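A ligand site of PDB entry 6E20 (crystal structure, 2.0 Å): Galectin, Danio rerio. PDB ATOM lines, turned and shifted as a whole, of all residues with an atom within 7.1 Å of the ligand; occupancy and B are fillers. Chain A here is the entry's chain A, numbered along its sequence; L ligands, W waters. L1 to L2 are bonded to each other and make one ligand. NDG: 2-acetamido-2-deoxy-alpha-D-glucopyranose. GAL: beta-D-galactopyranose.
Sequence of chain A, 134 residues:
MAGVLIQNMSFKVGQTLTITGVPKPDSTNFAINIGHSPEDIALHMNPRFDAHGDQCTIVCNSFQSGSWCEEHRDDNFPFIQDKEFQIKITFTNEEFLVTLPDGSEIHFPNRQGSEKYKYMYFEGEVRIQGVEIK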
ATOM      1  N   ASN A  29      -2.707 -10.306   7.407  1.00  0.00           N
ATOM      2  CA  ASN A  29      -1.936 -10.804   8.575  1.00  0.00           C
ATOM      3  C   ASN A  29      -2.872 -10.957   9.771  1.00  0.00           C
ATOM      4  O   ASN A  29      -4.042 -10.552   9.662  1.00  0.00           O
ATOM      5  CB  ASN A  29      -0.777  -9.862   8.933  1.00  0.00           C
ATOM      6  CG  ASN A  29      -1.280  -8.564   9.518  1.00  0.00           C
ATOM      7  OD1 ASN A  29      -1.946  -7.795   8.829  1.00  0.00           O
ATOM      8  ND2 ASN A  29      -0.967  -8.327  10.782  1.00  0.00           N
ATOM      9  N   ALA A  31      -2.234 -11.424  14.435  1.00  0.00           N
ATOM     10  CA  ALA A  31      -1.292 -11.317  15.574  1.00  0.00           C
ATOM     11  C   ALA A  31      -1.909 -11.906  16.841  1.00  0.00           C
ATOM     12  O   ALA A  31      -3.130 -11.655  17.111  1.00  0.00           O
ATOM     13  CB  ALA A  31      -0.899  -9.880  15.782  1.00  0.00           C
ATOM     14  N   HIS A  44       4.617 -11.062  20.721  1.00  0.00           N
ATOM     15  CA  HIS A  44       3.803 -10.676  19.530  1.00  0.00           C
ATOM     16  C   HIS A  44       4.170 -11.644  18.409  1.00  0.00           C
ATOM     17  O   HIS A  44       5.338 -11.639  17.954  1.00  0.00           O
ATOM     18  CB  HIS A  44       4.046  -9.198  19.203  1.00  0.00           C
ATOM     19  CG  HIS A  44       3.494  -8.739  17.893  1.00  0.00           C
ATOM     20  ND1 HIS A  44       2.194  -8.262  17.751  1.00  0.00           N
ATOM     21  CD2 HIS A  44       4.073  -8.615  16.676  1.00  0.00           C
ATOM     22  CE1 HIS A  44       1.996  -7.870  16.499  1.00  0.00           C
ATOM     23  NE2 HIS A  44       3.140  -8.058  15.820  1.00  0.00           N
ATOM     24  N   ASN A  46       3.207 -12.772  14.694  1.00  0.00           N
ATOM     25  CA  ASN A  46       2.518 -11.994  13.635  1.00  0.00           C
ATOM     26  C   ASN A  46       2.733 -12.688  12.294  1.00  0.00           C
ATOM     27  O   ASN A  46       3.633 -12.327  11.542  1.00  0.00           O
ATOM     28  CB  ASN A  46       2.965 -10.531  13.671  1.00  0.00           C
ATOM     29  CG  ASN A  46       2.230  -9.660  12.671  1.00  0.00           C
ATOM     30  OD1 ASN A  46       2.757  -8.650  12.205  1.00  0.00           O
ATOM     31  ND2 ASN A  46       1.016 -10.058  12.326  1.00  0.00           N
ATOM     32  N   ARG A  48       2.268 -13.100   8.540  1.00  0.00           N
ATOM     33  CA  ARG A  48       1.991 -12.116   7.471  1.00  0.00           C
ATOM     34  C   ARG A  48       1.818 -12.871   6.154  1.00  0.00           C
ATOM     35  O   ARG A  48       2.822 -13.378   5.649  1.00  0.00           O
ATOM     36  CB  ARG A  48       3.098 -11.068   7.388  1.00  0.00           C
ATOM     37  CG  ARG A  48       3.278 -10.312   8.698  1.00  0.00           C
ATOM     38  CD  ARG A  48       4.348  -9.243   8.644  1.00  0.00           C
ATOM     39  NE  ARG A  48       4.454  -8.526   9.909  1.00  0.00           N
ATOM     40  CZ  ARG A  48       5.325  -7.547  10.164  1.00  0.00           C
ATOM     41  NH1 ARG A  48       6.174  -7.150   9.229  1.00  0.00           N
ATOM     42  NH2 ARG A  48       5.341  -6.956  11.353  1.00  0.00           N
ATOM     43  N   ALA A  51       1.853  -8.264   4.297  1.00  0.00           N
ATOM     44  CA  ALA A  51       1.753  -7.010   5.085  1.00  0.00           C
ATOM     45  C   ALA A  51       3.144  -6.461   5.352  1.00  0.00           C
ATOM     46  O   ALA A  51       4.057  -7.264   5.633  1.00  0.00           O
ATOM     47  CB  ALA A  51       0.990  -7.270   6.361  1.00  0.00           C
ATOM     48  N   HIS A  52       3.318  -5.142   5.223  1.00  0.00           N
ATOM     49  CA  HIS A  52       4.544  -4.422   5.617  1.00  0.00           C
ATOM     50  C   HIS A  52       5.710  -4.814   4.700  1.00  0.00           C
ATOM     51  O   HIS A  52       6.901  -4.735   5.143  1.00  0.00           O
ATOM     52  CB  HIS A  52       4.799  -4.679   7.121  1.00  0.00           C
ATOM     53  CG  HIS A  52       3.624  -4.327   7.986  1.00  0.00           C
ATOM     54  ND1 HIS A  52       3.031  -5.231   8.830  1.00  0.00           N
ATOM     55  CD2 HIS A  52       2.904  -3.189   8.089  1.00  0.00           C
ATOM     56  CE1 HIS A  52       2.030  -4.649   9.453  1.00  0.00           C
ATOM     57  NE2 HIS A  52       1.928  -3.405   9.003  1.00  0.00           N
ATOM     58  N   ASP A  54       6.133  -7.846   3.565  1.00  0.00           N
ATOM     59  CA  ASP A  54       6.440  -9.274   3.880  1.00  0.00           C
ATOM     60  C   ASP A  54       5.322 -10.179   3.326  1.00  0.00           C
ATOM     61  O   ASP A  54       4.178  -9.890   3.571  1.00  0.00           O
ATOM     62  CB  ASP A  54       6.570  -9.469   5.396  1.00  0.00           C
ATOM     63  CG  ASP A  54       7.774  -8.746   6.018  1.00  0.00           C
ATOM     64  OD1 ASP A  54       8.840  -8.741   5.401  1.00  0.00           O
ATOM     65  OD2 ASP A  54       7.642  -8.220   7.136  1.00  0.00           O
ATOM     66  N   VAL A  59       6.569 -12.928  11.821  1.00  0.00           N
ATOM     67  CA  VAL A  59       7.374 -11.921  12.576  1.00  0.00           C
ATOM     68  C   VAL A  59       7.038 -12.095  14.051  1.00  0.00           C
ATOM     69  O   VAL A  59       5.855 -11.942  14.414  1.00  0.00           O
ATOM     70  CB  VAL A  59       7.105 -10.497  12.093  1.00  0.00           C
ATOM     71  CG1 VAL A  59       7.685  -9.474  13.065  1.00  0.00           C
ATOM     72  CG2 VAL A  59       7.635 -10.294  10.677  1.00  0.00           C
ATOM     73  N   CYS A  60       8.058 -12.331  14.872  1.00  0.00           N
ATOM     74  CA  CYS A  60       7.920 -12.383  16.343  1.00  0.00           C
ATOM     75  C   CYS A  60       8.724 -11.224  16.943  1.00  0.00           C
ATOM     76  O   CYS A  60       9.796 -10.875  16.437  1.00  0.00           O
ATOM     77  CB  CYS A  60       8.384 -13.710  16.926  1.00  0.00           C
ATOM     78  SG  CYS A  60       7.394 -15.143  16.406  1.00  0.00           S
ATOM     79  N   ASN A  61       8.180 -10.629  17.990  1.00  0.00           N
ATOM     80  CA  ASN A  61       8.805  -9.446  18.625  1.00  0.00           C
ATOM     81  C   ASN A  61       8.167  -9.240  19.998  1.00  0.00           C
ATOM     82  O   ASN A  61       7.249 -10.000  20.372  1.00  0.00           O
ATOM     83  CB  ASN A  61       8.677  -8.213  17.720  1.00  0.00           C
ATOM     84  CG  ASN A  61       9.726  -7.162  18.005  1.00  0.00           C
ATOM     85  OD1 ASN A  61      10.439  -7.263  19.001  1.00  0.00           O
ATOM     86  ND2 ASN A  61       9.857  -6.200  17.121  1.00  0.00           N
ATOM     87  N   SER A  62       8.658  -8.253  20.722  1.00  0.00           N
ATOM     88  CA  SER A  62       8.141  -7.829  22.030  1.00  0.00           C
ATOM     89  C   SER A  62       8.019  -6.307  22.037  1.00  0.00           C
ATOM     90  O   SER A  62       8.710  -5.679  21.226  1.00  0.00           O
ATOM     91  CB  SER A  62       9.044  -8.327  23.125  1.00  0.00           C
ATOM     92  OG  SER A  62      10.350  -7.813  22.928  1.00  0.00           O
ATOM     93  N   TRP A  68       8.909  -1.275  19.830  1.00  0.00           N
ATOM     94  CA  TRP A  68       9.180  -2.671  19.387  1.00  0.00           C
ATOM     95  C   TRP A  68      10.660  -2.982  19.609  1.00  0.00           C
ATOM     96  O   TRP A  68      11.500  -2.064  19.460  1.00  0.00           O
ATOM     97  CB  TRP A  68       8.775  -2.854  17.916  1.00  0.00           C
ATOM     98  CG  TRP A  68       7.297  -2.821  17.704  1.00  0.00           C
ATOM     99  CD1 TRP A  68       6.575  -1.813  17.129  1.00  0.00           C
ATOM    100  CD2 TRP A  68       6.353  -3.821  18.114  1.00  0.00           C
ATOM    101  NE1 TRP A  68       5.243  -2.115  17.139  1.00  0.00           N
ATOM    102  CE2 TRP A  68       5.071  -3.339  17.743  1.00  0.00           C
ATOM    103  CE3 TRP A  68       6.462  -5.055  18.751  1.00  0.00           C
ATOM    104  CZ2 TRP A  68       3.911  -4.069  17.970  1.00  0.00           C
ATOM    105  CZ3 TRP A  68       5.309  -5.782  18.971  1.00  0.00           C
ATOM    106  CH2 TRP A  68       4.057  -5.281  18.607  1.00  0.00           C
ATOM    107  N   YCM A  69      10.991  -4.223  19.968  1.00  0.00           N
ATOM    108  CA  YCM A  69      12.399  -4.680  20.184  1.00  0.00           C
ATOM    109  CB  YCM A  69      12.414  -5.594  21.393  1.00  0.00           C
ATOM    110  SG  YCM A  69      14.073  -6.143  21.874  1.00  0.00           S
ATOM    111  CD  YCM A  69      14.824  -4.589  22.441  1.00  0.00           C
ATOM    112  CE  YCM A  69      16.053  -4.292  21.621  1.00  0.00           C
ATOM    113  OZ1 YCM A  69      15.964  -3.584  20.618  1.00  0.00           O
ATOM    114  NZ2 YCM A  69      17.164  -4.875  22.019  1.00  0.00           N
ATOM    115  C   YCM A  69      12.878  -5.293  18.859  1.00  0.00           C
ATOM    116  O   YCM A  69      12.325  -4.914  17.814  1.00  0.00           O
ATOM    117  N   GLU A  70      13.847  -6.216  18.878  1.00  0.00           N
ATOM    118  CA  GLU A  70      14.376  -6.820  17.622  1.00  0.00           C
ATOM    119  C   GLU A  70      13.456  -7.949  17.133  1.00  0.00           C
ATOM    120  O   GLU A  70      13.094  -8.872  17.941  1.00  0.00           O
ATOM    121  CB  GLU A  70      15.792  -7.318  17.845  1.00  0.00           C
ATOM    122  CG  GLU A  70      16.356  -8.073  16.660  1.00  0.00           C
ATOM    123  CD  GLU A  70      17.753  -8.582  16.933  1.00  0.00           C
ATOM    124  OE1 GLU A  70      18.680  -7.778  16.892  1.00  0.00           O
ATOM    125  OE2 GLU A  70      17.882  -9.781  17.206  1.00  0.00           O
ATOM    126  N   GLU A  71      13.146  -7.946  15.837  1.00  0.00           N
ATOM    127  CA  GLU A  71      12.241  -8.966  15.224  1.00  0.00           C
ATOM    128  C   GLU A  71      12.999 -10.285  15.053  1.00  0.00           C
ATOM    129  O   GLU A  71      14.159 -10.238  14.648  1.00  0.00           O
ATOM    130  CB  GLU A  71      11.748  -8.509  13.857  1.00  0.00           C
ATOM    131  CG  GLU A  71      10.782  -7.351  13.937  1.00  0.00           C
ATOM    132  CD  GLU A  71      10.073  -6.975  12.645  1.00  0.00           C
ATOM    133  OE1 GLU A  71      10.452  -7.550  11.583  1.00  0.00           O
ATOM    134  OE2 GLU A  71       9.171  -6.101  12.706  1.00  0.00           O
ATOM    135  N   HIS A  72      12.269 -11.358  15.276  1.00  0.00           N
ATOM    136  CA  HIS A  72      12.682 -12.718  14.900  1.00  0.00           C
ATOM    137  C   HIS A  72      11.796 -13.066  13.691  1.00  0.00           C
ATOM    138  O   HIS A  72      10.585 -13.071  13.838  1.00  0.00           O
ATOM    139  CB  HIS A  72      12.603 -13.681  16.070  1.00  0.00           C
ATOM    140  CG  HIS A  72      13.681 -13.481  17.072  1.00  0.00           C
ATOM    141  ND1 HIS A  72      14.461 -14.499  17.511  1.00  0.00           N
ATOM    142  CD2 HIS A  72      14.099 -12.390  17.713  1.00  0.00           C
ATOM    143  CE1 HIS A  72      15.304 -14.051  18.389  1.00  0.00           C
ATOM    144  NE2 HIS A  72      15.106 -12.775  18.528  1.00  0.00           N
ATOM    145  N   ARG A  73      12.396 -13.282  12.524  1.00  0.00           N
ATOM    146  CA  ARG A  73      11.649 -13.527  11.270  1.00  0.00           C
ATOM    147  C   ARG A  73      11.835 -14.972  10.768  1.00  0.00           C
ATOM    148  O   ARG A  73      12.937 -15.439  10.771  1.00  0.00           O
ATOM    149  CB  ARG A  73      12.009 -12.422  10.288  1.00  0.00           C
ATOM    150  CG  ARG A  73      11.611 -11.047  10.800  1.00  0.00           C
ATOM    151  CD  ARG A  73      12.263  -9.838  10.180  1.00  0.00           C
ATOM    152  NE  ARG A  73      11.946  -9.849   8.785  1.00  0.00           N
ATOM    153  CZ  ARG A  73      10.878  -9.322   8.235  1.00  0.00           C
ATOM    154  NH1 ARG A  73       9.985  -8.659   8.951  1.00  0.00           N
ATOM    155  NH2 ARG A  73      10.729  -9.403   6.942  1.00  0.00           N
ATOM    156  N   GLU A 123      -5.253  -9.771  17.076  1.00  0.00           N
ATOM    157  CA  GLU A 123      -5.398  -8.637  16.134  1.00  0.00           C
ATOM    158  C   GLU A 123      -5.517  -9.196  14.720  1.00  0.00           C
ATOM    159  O   GLU A 123      -4.965 -10.291  14.447  1.00  0.00           O
ATOM    160  CB  GLU A 123      -4.177  -7.709  16.170  1.00  0.00           C
ATOM    161  CG  GLU A 123      -3.734  -7.290  17.557  1.00  0.00           C
ATOM    162  CD  GLU A 123      -2.669  -6.199  17.563  1.00  0.00           C
ATOM    163  OE1 GLU A 123      -1.458  -6.520  17.317  1.00  0.00           O
ATOM    164  OE2 GLU A 123      -3.052  -5.014  17.761  1.00  0.00           O
HETATM  165  C1  NDG L   1      10.030  -2.330   9.958  1.00  0.00           C
HETATM  166  C2  NDG L   1       9.736  -3.824  10.080  1.00  0.00           C
HETATM  167  C3  NDG L   1       8.239  -4.072  10.279  1.00  0.00           C
HETATM  168  C4  NDG L   1       7.756  -3.246  11.468  1.00  0.00           C
HETATM  169  C5  NDG L   1       8.131  -1.779  11.287  1.00  0.00           C
HETATM  170  C6  NDG L   1       7.715  -0.897  12.460  1.00  0.00           C
HETATM  171  C7  NDG L   1      11.511  -5.158   9.059  1.00  0.00           C
HETATM  172  C8  NDG L   1      11.994  -6.016   7.932  1.00  0.00           C
HETATM  173  O5  NDG L   1       9.528  -1.626  11.071  1.00  0.00           O
HETATM  174  O3  NDG L   1       8.027  -5.487  10.542  1.00  0.00           O
HETATM  175  O4  NDG L   1       6.334  -3.366  11.582  1.00  0.00           O
HETATM  176  O6  NDG L   1       8.307  -1.282  13.690  1.00  0.00           O
HETATM  177  O7  NDG L   1      12.230  -5.013  10.045  1.00  0.00           O
HETATM  178  N2  NDG L   1      10.292  -4.580   8.960  1.00  0.00           N
HETATM  179  O1  NDG L   1       9.434  -1.825   8.751  1.00  0.00           O
HETATM  180  C1  GAL L   2       5.860  -3.607  12.894  1.00  0.00           C
HETATM  181  C2  GAL L   2       4.340  -3.546  12.810  1.00  0.00           C
HETATM  182  C3  GAL L   2       3.672  -3.946  14.105  1.00  0.00           C
HETATM  183  C4  GAL L   2       4.290  -5.214  14.673  1.00  0.00           C
HETATM  184  C5  GAL L   2       5.828  -5.131  14.679  1.00  0.00           C
HETATM  185  C6  GAL L   2       6.578  -6.397  15.075  1.00  0.00           C
HETATM  186  O2  GAL L   2       3.905  -2.220  12.461  1.00  0.00           O
HETATM  187  O3  GAL L   2       2.310  -4.214  13.773  1.00  0.00           O
HETATM  188  O4  GAL L   2       3.826  -6.319  13.878  1.00  0.00           O
HETATM  189  O5  GAL L   2       6.282  -4.899  13.373  1.00  0.00           O
HETATM  190  O6  GAL L   2       7.995  -6.197  14.969  1.00  0.00           O
HETATM  191  O   HOH W   1       9.936  -3.649  14.376  1.00  0.00           O
HETATM  192  O   HOH W   2       1.432  -6.310  12.567  1.00  0.00           O
HETATM  193  O   HOH W   3      12.277  -4.111  12.750  1.00  0.00           O
HETATM  194  O   HOH W   4       8.580  -5.423   6.990  1.00  0.00           O
HETATM  195  O   HOH W   5       8.646   0.657  15.497  1.00  0.00           O
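The side-chain amide oxygen of Asn 46 lies within hydrogen-bond range of an oxygen (O4) of GAL L2, 3.1 Å away. ND2 of Asn 61 lies within hydrogen-bond range of O6 of GAL L2 (2.8 Å). An oxygen (O3) of NDG L1 lies within hydrogen-bond range of the guanidinium group (NH1) of Arg 48 (2.8 Å). NE2 of His 44 sits at hydrogen-bond distance from O4 of GAL L2 (2.7 Å). OE2 of Glu 71 is in hydrogen-bond range of O3 of NDG L1, 2.5 Å away.
The side-chain amide nitrogen (ND2) of Asn 61 sits at hydrogen-bond distance from O of YCM 69. The side-chain carboxylate (OD2) of Asp 54 lies within salt-bridge range of the guanidinium group (NH1) of Arg 48 (2.8 Å). The side-chain carboxylate (OD1) of Asp 54 lies within salt-bridge range of the guanidinium group (NH2) of Arg 73 (2.5 Å). The guanidinium group of Arg 48 is in hydrogen-bond range of the side-chain amide oxygen of Asn 46, at 2.9 Å. The side-chain amide nitrogen of Asn 46 lies close to the side-chain amide nitrogen of Asn 29, 3.1 Å away. The backbone NH of Asn 46 is in hydrogen-bond range of the backbone carbonyl oxygen of Val 59, 2.8 Å away. OD1 of Asn 61 lies close to O of Glu 70. The backbone NH (N) of His 44 is in hydrogen-bond range of the backbone carbonyl oxygen (O) of Asn 61, 2.9 Å away.
Val 59 touches the ligand. Trp 68 touches the ligand. NH1 of Arg 73 touches C8 of NDG L1 (3.5 Å). Along chain A the residues within 4 Å of the ligand span positions 44 to 73. The nearest printed residue that does not touch the ligand is His 52 (4.2 Å).
Water W2 bridges an oxygen (O3) of GAL L2 (2.6 Å) and the side-chain amide oxygen (OD1) of Asn 46 (2.7 Å). Water W4 lies within hydrogen-bond range of the backbone carbonyl oxygen (O) of His 52, a nitrogen (N2) of NDG L1 and the side-chain carboxylate (OD2) of Asp 54. Water W1 lies within hydrogen-bond range of an oxygen (O6) of NDG L1 (3.0 Å) and the side-chain carboxylate (OE2) of Glu 71 (3.1 Å).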
